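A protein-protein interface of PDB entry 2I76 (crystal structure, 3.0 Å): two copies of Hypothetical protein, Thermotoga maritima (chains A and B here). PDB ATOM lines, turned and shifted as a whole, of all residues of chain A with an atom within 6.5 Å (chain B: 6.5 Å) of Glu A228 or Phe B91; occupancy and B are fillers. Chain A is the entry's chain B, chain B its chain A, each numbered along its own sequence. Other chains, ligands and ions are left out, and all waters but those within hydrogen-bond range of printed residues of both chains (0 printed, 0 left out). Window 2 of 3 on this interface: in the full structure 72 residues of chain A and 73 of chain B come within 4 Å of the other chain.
N of Leu B162 is in hydrogen-bond range of OE2 of Glu A229 (3.4 Å).
The side-chain hydroxyl of Ser B89 lies within hydrogen-bond range of the backbone NH of Phe B91, at 3.1 Å. The side-chain amide nitrogen (NE2) of Gln A224 lies within hydrogen-bond range of the side-chain carboxylate (OE1) of Glu A228 (3.0 Å).
CE2 of Phe B91 touches CG2 of Val A225, at 3.7 Å. OE2 of Glu A228 touches CZ of Phe B91 (3.6 Å). Glu A229 touches His B161 (OE2 to CD2, 2.8 Å). Glu A232 touches Lys B158 (OE2 to CB, 3.8 Å). CG of Glu A232 touches CA of Ala B159, 3.6 Å away. Glu A232 touches Leu B162 (C to CD1, 3.8 Å). Tyr A233 touches Leu B162.
Tyr A243 touches none of the printed residues of chain B. Of chain A, only Val A225 (3.7 Å) and Glu A228 (3.6 Å) come within 4 Å of Phe B91. Printed residues of chain A within 4 Å of Lys B158: Glu A232. Of the printed residues of chain A, Ala B159 touches Glu A232 (3.6 Å). The nearest residue of chain B that does not touch Glu A228 is Lys B158 (4.1 Å). The nearest residue of chain A that does not touch Phe B91 is Glu A229 (4.2 Å). The nearest printed residue of chain A that does not touch His B161 is Val A225 (4.2 Å).
Along chain A the printed residues that touch a printed residue of chain B span positions 225 to 233. Hydrophobic or aromatic side chains of chain B that line the printed part of chain A: Phe B91, His B161 and Leu B162.
No position is printed for both chains. Of the 8 pairs that touch across the chains among the printed residues, none has its exchanged pair printed and touching as well.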
ATOM      1  N   TRP A 223      34.152 -10.052  28.385  1.00  0.00           N
ATOM      2  CA  TRP A 223      34.786  -9.184  27.428  1.00  0.00           C
ATOM      3  C   TRP A 223      33.789  -8.766  26.364  1.00  0.00           C
ATOM      4  O   TRP A 223      34.041  -7.829  25.603  1.00  0.00           O
ATOM      5  CB  TRP A 223      35.981  -9.902  26.791  1.00  0.00           C
ATOM      6  CG  TRP A 223      35.673 -10.494  25.464  1.00  0.00           C
ATOM      7  CD1 TRP A 223      36.203 -10.122  24.269  1.00  0.00           C
ATOM      8  CD2 TRP A 223      34.651 -11.454  25.167  1.00  0.00           C
ATOM      9  NE1 TRP A 223      35.565 -10.769  23.241  1.00  0.00           N
ATOM     10  CE2 TRP A 223      34.606 -11.597  23.764  1.00  0.00           C
ATOM     11  CE3 TRP A 223      33.765 -12.201  25.948  1.00  0.00           C
ATOM     12  CZ2 TRP A 223      33.707 -12.452  23.122  1.00  0.00           C
ATOM     13  CZ3 TRP A 223      32.871 -13.052  25.308  1.00  0.00           C
ATOM     14  CH2 TRP A 223      32.851 -13.169  23.908  1.00  0.00           C
ATOM     15  N   GLN A 224      32.656  -9.456  26.294  1.00  0.00           N
ATOM     16  CA  GLN A 224      31.684  -9.095  25.276  1.00  0.00           C
ATOM     17  C   GLN A 224      30.947  -7.885  25.758  1.00  0.00           C
ATOM     18  O   GLN A 224      30.344  -7.161  24.971  1.00  0.00           O
ATOM     19  CB  GLN A 224      30.687 -10.208  25.005  1.00  0.00           C
ATOM     20  CG  GLN A 224      30.051 -10.053  23.654  1.00  0.00           C
ATOM     21  CD  GLN A 224      28.821 -10.878  23.484  1.00  0.00           C
ATOM     22  OE1 GLN A 224      28.757 -12.020  23.925  1.00  0.00           O
ATOM     23  NE2 GLN A 224      27.829 -10.313  22.824  1.00  0.00           N
ATOM     24  N   VAL A 225      30.996  -7.679  27.070  1.00  0.00           N
ATOM     25  CA  VAL A 225      30.364  -6.518  27.686  1.00  0.00           C
ATOM     26  C   VAL A 225      31.336  -5.336  27.520  1.00  0.00           C
ATOM     27  O   VAL A 225      30.918  -4.231  27.183  1.00  0.00           O
ATOM     28  CB  VAL A 225      30.028  -6.778  29.206  1.00  0.00           C
ATOM     29  CG1 VAL A 225      29.732  -5.481  29.907  1.00  0.00           C
ATOM     30  CG2 VAL A 225      28.811  -7.682  29.327  1.00  0.00           C
ATOM     31  N   VAL A 226      32.630  -5.572  27.719  1.00  0.00           N
ATOM     32  CA  VAL A 226      33.583  -4.492  27.562  1.00  0.00           C
ATOM     33  C   VAL A 226      33.608  -4.010  26.121  1.00  0.00           C
ATOM     34  O   VAL A 226      33.632  -2.807  25.860  1.00  0.00           O
ATOM     35  CB  VAL A 226      34.993  -4.907  27.960  1.00  0.00           C
ATOM     36  CG1 VAL A 226      35.983  -3.849  27.499  1.00  0.00           C
ATOM     37  CG2 VAL A 226      35.084  -5.067  29.471  1.00  0.00           C
ATOM     38  N   GLU A 227      33.589  -4.947  25.183  1.00  0.00           N
ATOM     39  CA  GLU A 227      33.613  -4.610  23.765  1.00  0.00           C
ATOM     40  C   GLU A 227      32.326  -3.921  23.301  1.00  0.00           C
ATOM     41  O   GLU A 227      32.373  -2.908  22.603  1.00  0.00           O
ATOM     42  CB  GLU A 227      33.881  -5.881  22.942  1.00  0.00           C
ATOM     43  CG  GLU A 227      33.861  -5.728  21.408  1.00  0.00           C
ATOM     44  CD  GLU A 227      34.785  -4.629  20.863  1.00  0.00           C
ATOM     45  OE1 GLU A 227      35.747  -4.218  21.555  1.00  0.00           O
ATOM     46  OE2 GLU A 227      34.554  -4.181  19.718  1.00  0.00           O
ATOM     47  N   GLU A 228      31.171  -4.455  23.681  1.00  0.00           N
ATOM     48  CA  GLU A 228      29.931  -3.826  23.260  1.00  0.00           C
ATOM     49  C   GLU A 228      29.809  -2.423  23.850  1.00  0.00           C
ATOM     50  O   GLU A 228      29.248  -1.527  23.219  1.00  0.00           O
ATOM     51  CB  GLU A 228      28.723  -4.699  23.627  1.00  0.00           C
ATOM     52  CG  GLU A 228      28.286  -5.585  22.463  1.00  0.00           C
ATOM     53  CD  GLU A 228      27.273  -6.666  22.821  1.00  0.00           C
ATOM     54  OE1 GLU A 228      26.997  -7.531  21.958  1.00  0.00           O
ATOM     55  OE2 GLU A 228      26.743  -6.673  23.948  1.00  0.00           O
ATOM     56  N   GLU A 229      30.355  -2.222  25.047  1.00  0.00           N
ATOM     57  CA  GLU A 229      30.303  -0.908  25.683  1.00  0.00           C
ATOM     58  C   GLU A 229      31.361   0.038  25.096  1.00  0.00           C
ATOM     59  O   GLU A 229      31.330   1.255  25.339  1.00  0.00           O
ATOM     60  CB  GLU A 229      30.482  -1.030  27.200  1.00  0.00           C
ATOM     61  CG  GLU A 229      29.268  -1.595  27.918  1.00  0.00           C
ATOM     62  CD  GLU A 229      29.541  -1.895  29.386  1.00  0.00           C
ATOM     63  OE1 GLU A 229      30.511  -2.616  29.682  1.00  0.00           O
ATOM     64  OE2 GLU A 229      28.790  -1.419  30.256  1.00  0.00           O
ATOM     65  N   ARG A 230      32.298  -0.506  24.327  1.00  0.00           N
ATOM     66  CA  ARG A 230      33.281   0.364  23.721  1.00  0.00           C
ATOM     67  C   ARG A 230      32.579   1.068  22.570  1.00  0.00           C
ATOM     68  O   ARG A 230      32.828   2.247  22.307  1.00  0.00           O
ATOM     69  CB  ARG A 230      34.479  -0.407  23.182  1.00  0.00           C
ATOM     70  CG  ARG A 230      35.751   0.423  23.243  1.00  0.00           C
ATOM     71  CD  ARG A 230      36.822  -0.013  22.273  1.00  0.00           C
ATOM     72  NE  ARG A 230      36.618   0.597  20.963  1.00  0.00           N
ATOM     73  CZ  ARG A 230      37.468   0.501  19.942  1.00  0.00           C
ATOM     74  NH1 ARG A 230      38.601  -0.186  20.078  1.00  0.00           N
ATOM     75  NH2 ARG A 230      37.181   1.086  18.781  1.00  0.00           N
ATOM     76  N   ARG A 231      31.696   0.342  21.889  1.00  0.00           N
ATOM     77  CA  ARG A 231      30.945   0.901  20.760  1.00  0.00           C
ATOM     78  C   ARG A 231      29.919   1.901  21.285  1.00  0.00           C
ATOM     79  O   ARG A 231      29.621   2.911  20.641  1.00  0.00           O
ATOM     80  CB  ARG A 231      30.235  -0.225  19.980  1.00  0.00           C
ATOM     81  N   GLU A 232      29.398   1.606  22.475  1.00  0.00           N
ATOM     82  CA  GLU A 232      28.391   2.427  23.137  1.00  0.00           C
ATOM     83  C   GLU A 232      29.073   3.670  23.676  1.00  0.00           C
ATOM     84  O   GLU A 232      28.459   4.726  23.796  1.00  0.00           O
ATOM     85  CB  GLU A 232      27.736   1.622  24.263  1.00  0.00           C
ATOM     86  CG  GLU A 232      26.475   2.243  24.840  1.00  0.00           C
ATOM     87  CD  GLU A 232      25.365   2.458  23.807  1.00  0.00           C
ATOM     88  OE1 GLU A 232      25.382   3.496  23.108  1.00  0.00           O
ATOM     89  OE2 GLU A 232      24.474   1.583  23.692  1.00  0.00           O
ATOM     90  N   TYR A 233      30.355   3.534  24.003  1.00  0.00           N
ATOM     91  CA  TYR A 233      31.135   4.664  24.493  1.00  0.00           C
ATOM     92  C   TYR A 233      31.368   5.574  23.288  1.00  0.00           C
ATOM     93  O   TYR A 233      31.099   6.781  23.333  1.00  0.00           O
ATOM     94  CB  TYR A 233      32.485   4.190  25.034  1.00  0.00           C
ATOM     95  CG  TYR A 233      33.345   5.290  25.615  1.00  0.00           C
ATOM     96  CD1 TYR A 233      33.402   5.495  26.984  1.00  0.00           C
ATOM     97  CD2 TYR A 233      34.079   6.149  24.787  1.00  0.00           C
ATOM     98  CE1 TYR A 233      34.162   6.528  27.524  1.00  0.00           C
ATOM     99  CE2 TYR A 233      34.844   7.190  25.318  1.00  0.00           C
ATOM    100  CZ  TYR A 233      34.875   7.374  26.691  1.00  0.00           C
ATOM    101  OH  TYR A 233      35.575   8.424  27.244  1.00  0.00           O
ATOM    102  N   TYR A 243      38.284   5.439  27.469  1.00  0.00           N
ATOM    103  CA  TYR A 243      37.703   4.138  27.741  1.00  0.00           C
ATOM    104  C   TYR A 243      38.772   3.056  27.591  1.00  0.00           C
ATOM    105  O   TYR A 243      38.994   2.258  28.499  1.00  0.00           O
ATOM    106  CB  TYR A 243      36.576   3.863  26.745  1.00  0.00           C
ATOM    107  CG  TYR A 243      35.874   2.559  26.984  1.00  0.00           C
ATOM    108  CD1 TYR A 243      34.768   2.493  27.828  1.00  0.00           C
ATOM    109  CD2 TYR A 243      36.346   1.377  26.423  1.00  0.00           C
ATOM    110  CE1 TYR A 243      34.144   1.282  28.116  1.00  0.00           C
ATOM    111  CE2 TYR A 243      35.734   0.147  26.707  1.00  0.00           C
ATOM    112  CZ  TYR A 243      34.629   0.111  27.557  1.00  0.00           C
ATOM    113  OH  TYR A 243      34.008  -1.084  27.862  1.00  0.00           O
ATOM    114  N   ASP B  68      23.800 -12.848  35.643  1.00  0.00           N
ATOM    115  CA  ASP B  68      23.417 -12.385  34.308  1.00  0.00           C
ATOM    116  C   ASP B  68      23.597 -13.465  33.235  1.00  0.00           C
ATOM    117  O   ASP B  68      22.982 -13.425  32.160  1.00  0.00           O
ATOM    118  CB  ASP B  68      24.278 -11.176  33.910  1.00  0.00           C
ATOM    119  CG  ASP B  68      23.635  -9.853  34.257  1.00  0.00           C
ATOM    120  OD1 ASP B  68      23.671  -9.453  35.432  1.00  0.00           O
ATOM    121  OD2 ASP B  68      23.087  -9.214  33.344  1.00  0.00           O
ATOM    122  N   HIS B  87      14.099  -9.493  35.756  1.00  0.00           N
ATOM    123  CA  HIS B  87      15.433  -9.765  36.273  1.00  0.00           C
ATOM    124  C   HIS B  87      16.003  -8.419  36.703  1.00  0.00           C
ATOM    125  O   HIS B  87      15.425  -7.361  36.423  1.00  0.00           O
ATOM    126  CB  HIS B  87      16.336 -10.457  35.240  1.00  0.00           C
ATOM    127  CG  HIS B  87      16.574  -9.655  34.004  1.00  0.00           C
ATOM    128  ND1 HIS B  87      17.267  -8.467  34.011  1.00  0.00           N
ATOM    129  CD2 HIS B  87      16.189  -9.860  32.723  1.00  0.00           C
ATOM    130  CE1 HIS B  87      17.295  -7.970  32.787  1.00  0.00           C
ATOM    131  NE2 HIS B  87      16.649  -8.796  31.987  1.00  0.00           N
ATOM    132  N   CYS B  88      17.134  -8.450  37.394  1.00  0.00           N
ATOM    133  CA  CYS B  88      17.720  -7.217  37.895  1.00  0.00           C
ATOM    134  C   CYS B  88      19.040  -6.871  37.231  1.00  0.00           C
ATOM    135  O   CYS B  88      19.816  -6.077  37.755  1.00  0.00           O
ATOM    136  CB  CYS B  88      17.911  -7.348  39.405  1.00  0.00           C
ATOM    137  SG  CYS B  88      16.592  -8.324  40.202  1.00  0.00           S
ATOM    138  N   SER B  89      19.296  -7.460  36.073  1.00  0.00           N
ATOM    139  CA  SER B  89      20.537  -7.200  35.365  1.00  0.00           C
ATOM    140  C   SER B  89      20.706  -5.727  35.024  1.00  0.00           C
ATOM    141  O   SER B  89      19.772  -5.082  34.511  1.00  0.00           O
ATOM    142  CB  SER B  89      20.590  -8.010  34.074  1.00  0.00           C
ATOM    143  OG  SER B  89      21.632  -7.542  33.241  1.00  0.00           O
ATOM    144  N   GLY B  90      21.906  -5.209  35.311  1.00  0.00           N
ATOM    145  CA  GLY B  90      22.225  -3.823  35.003  1.00  0.00           C
ATOM    146  C   GLY B  90      22.617  -3.672  33.540  1.00  0.00           C
ATOM    147  O   GLY B  90      22.553  -2.594  32.949  1.00  0.00           O
ATOM    148  N   PHE B  91      23.022  -4.778  32.937  1.00  0.00           N
ATOM    149  CA  PHE B  91      23.415  -4.741  31.548  1.00  0.00           C
ATOM    150  C   PHE B  91      22.311  -5.278  30.664  1.00  0.00           C
ATOM    151  O   PHE B  91      21.820  -4.581  29.777  1.00  0.00           O
ATOM    152  CB  PHE B  91      24.674  -5.569  31.337  1.00  0.00           C
ATOM    153  CG  PHE B  91      25.160  -5.569  29.924  1.00  0.00           C
ATOM    154  CD1 PHE B  91      25.622  -4.390  29.336  1.00  0.00           C
ATOM    155  CD2 PHE B  91      25.139  -6.743  29.167  1.00  0.00           C
ATOM    156  CE1 PHE B  91      26.063  -4.381  28.023  1.00  0.00           C
ATOM    157  CE2 PHE B  91      25.579  -6.748  27.854  1.00  0.00           C
ATOM    158  CZ  PHE B  91      26.040  -5.562  27.277  1.00  0.00           C
ATOM    159  N   LEU B  92      21.930  -6.527  30.925  1.00  0.00           N
ATOM    160  CA  LEU B  92      20.895  -7.219  30.160  1.00  0.00           C
ATOM    161  C   LEU B  92      19.533  -6.550  30.275  1.00  0.00           C
ATOM    162  O   LEU B  92      19.229  -5.880  31.270  1.00  0.00           O
ATOM    163  CB  LEU B  92      20.798  -8.688  30.598  1.00  0.00           C
ATOM    164  CG  LEU B  92      22.023  -9.577  30.332  1.00  0.00           C
ATOM    165  CD1 LEU B  92      21.970 -10.861  31.157  1.00  0.00           C
ATOM    166  CD2 LEU B  92      22.102  -9.876  28.852  1.00  0.00           C
ATOM    167  N   SER B  93      18.715  -6.749  29.244  1.00  0.00           N
ATOM    168  CA  SER B  93      17.382  -6.169  29.169  1.00  0.00           C
ATOM    169  C   SER B  93      16.283  -7.195  29.411  1.00  0.00           C
ATOM    170  O   SER B  93      16.481  -8.397  29.222  1.00  0.00           O
ATOM    171  CB  SER B  93      17.183  -5.549  27.788  1.00  0.00           C
ATOM    172  OG  SER B  93      15.942  -4.885  27.703  1.00  0.00           O
ATOM    173  N   HIS B 106      16.599  -2.709  38.286  1.00  0.00           N
ATOM    174  CA  HIS B 106      17.994  -2.642  38.688  1.00  0.00           C
ATOM    175  C   HIS B 106      18.371  -1.630  39.758  1.00  0.00           C
ATOM    176  O   HIS B 106      18.388  -0.417  39.506  1.00  0.00           O
ATOM    177  CB  HIS B 106      18.875  -2.413  37.452  1.00  0.00           C
ATOM    178  CG  HIS B 106      20.337  -2.358  37.769  1.00  0.00           C
ATOM    179  ND1 HIS B 106      20.995  -1.179  38.052  1.00  0.00           N
ATOM    180  CD2 HIS B 106      21.245  -3.348  37.940  1.00  0.00           C
ATOM    181  CE1 HIS B 106      22.245  -1.446  38.387  1.00  0.00           C
ATOM    182  NE2 HIS B 106      22.422  -2.754  38.328  1.00  0.00           N
ATOM    183  N   SER B 154      14.440  -0.369  26.505  1.00  0.00           N
ATOM    184  CA  SER B 154      15.235  -1.602  26.468  1.00  0.00           C
ATOM    185  C   SER B 154      16.445  -1.472  25.533  1.00  0.00           C
ATOM    186  O   SER B 154      17.467  -2.151  25.709  1.00  0.00           O
ATOM    187  CB  SER B 154      14.375  -2.783  26.003  1.00  0.00           C
ATOM    188  OG  SER B 154      13.453  -3.186  26.997  1.00  0.00           O
ATOM    189  N   LYS B 157      19.779   0.122  27.573  1.00  0.00           N
ATOM    190  CA  LYS B 157      20.260  -0.411  28.835  1.00  0.00           C
ATOM    191  C   LYS B 157      21.780  -0.549  28.855  1.00  0.00           C
ATOM    192  O   LYS B 157      22.398  -0.491  29.926  1.00  0.00           O
ATOM    193  CB  LYS B 157      19.585  -1.756  29.107  1.00  0.00           C
ATOM    194  CG  LYS B 157      19.638  -2.182  30.554  1.00  0.00           C
ATOM    195  CD  LYS B 157      18.458  -3.058  30.904  1.00  0.00           C
ATOM    196  CE  LYS B 157      18.467  -3.423  32.380  1.00  0.00           C
ATOM    197  NZ  LYS B 157      18.598  -2.217  33.228  1.00  0.00           N
ATOM    198  N   LYS B 158      22.376  -0.732  27.671  1.00  0.00           N
ATOM    199  CA  LYS B 158      23.837  -0.844  27.534  1.00  0.00           C
ATOM    200  C   LYS B 158      24.489   0.500  27.833  1.00  0.00           C
ATOM    201  O   LYS B 158      25.580   0.557  28.393  1.00  0.00           O
ATOM    202  CB  LYS B 158      24.229  -1.289  26.124  1.00  0.00           C
ATOM    203  CG  LYS B 158      24.055  -2.776  25.875  1.00  0.00           C
ATOM    204  CD  LYS B 158      24.535  -3.202  24.488  1.00  0.00           C
ATOM    205  CE  LYS B 158      23.718  -2.546  23.375  1.00  0.00           C
ATOM    206  NZ  LYS B 158      23.994  -3.131  22.025  1.00  0.00           N
ATOM    207  N   ALA B 159      23.823   1.581  27.439  1.00  0.00           N
ATOM    208  CA  ALA B 159      24.329   2.919  27.712  1.00  0.00           C
ATOM    209  C   ALA B 159      24.298   3.087  29.224  1.00  0.00           C
ATOM    210  O   ALA B 159      25.309   3.414  29.853  1.00  0.00           O
ATOM    211  CB  ALA B 159      23.442   3.960  27.064  1.00  0.00           C
ATOM    212  N   TYR B 160      23.120   2.848  29.790  1.00  0.00           N
ATOM    213  CA  TYR B 160      22.873   2.938  31.223  1.00  0.00           C
ATOM    214  C   TYR B 160      23.945   2.205  32.029  1.00  0.00           C
ATOM    215  O   TYR B 160      24.566   2.778  32.926  1.00  0.00           O
ATOM    216  CB  TYR B 160      21.505   2.342  31.488  1.00  0.00           C
ATOM    217  CG  TYR B 160      21.170   1.999  32.914  1.00  0.00           C
ATOM    218  CD1 TYR B 160      20.498   2.912  33.736  1.00  0.00           C
ATOM    219  CD2 TYR B 160      21.384   0.707  33.398  1.00  0.00           C
ATOM    220  CE1 TYR B 160      20.021   2.533  35.003  1.00  0.00           C
ATOM    221  CE2 TYR B 160      20.920   0.320  34.652  1.00  0.00           C
ATOM    222  CZ  TYR B 160      20.234   1.232  35.445  1.00  0.00           C
ATOM    223  OH  TYR B 160      19.726   0.814  36.652  1.00  0.00           O
ATOM    224  N   HIS B 161      24.163   0.935  31.706  1.00  0.00           N
ATOM    225  CA  HIS B 161      25.172   0.154  32.414  1.00  0.00           C
ATOM    226  C   HIS B 161      26.550   0.804  32.255  1.00  0.00           C
ATOM    227  O   HIS B 161      27.308   0.920  33.223  1.00  0.00           O
ATOM    228  CB  HIS B 161      25.200  -1.295  31.896  1.00  0.00           C
ATOM    229  CG  HIS B 161      26.219  -2.161  32.576  1.00  0.00           C
ATOM    230  ND1 HIS B 161      26.291  -2.293  33.948  1.00  0.00           N
ATOM    231  CD2 HIS B 161      27.213  -2.934  32.072  1.00  0.00           C
ATOM    232  CE1 HIS B 161      27.285  -3.109  34.261  1.00  0.00           C
ATOM    233  NE2 HIS B 161      27.860  -3.512  33.141  1.00  0.00           N
ATOM    234  N   LEU B 162      26.866   1.230  31.031  1.00  0.00           N
ATOM    235  CA  LEU B 162      28.143   1.883  30.750  1.00  0.00           C
ATOM    236  C   LEU B 162      28.354   2.936  31.842  1.00  0.00           C
ATOM    237  O   LEU B 162      29.360   2.922  32.554  1.00  0.00           O
ATOM    238  CB  LEU B 162      28.099   2.559  29.375  1.00  0.00           C
ATOM    239  CG  LEU B 162      29.421   2.723  28.614  1.00  0.00           C
ATOM    240  CD1 LEU B 162      29.201   3.690  27.464  1.00  0.00           C
ATOM    241  CD2 LEU B 162      30.517   3.237  29.536  1.00  0.00           C
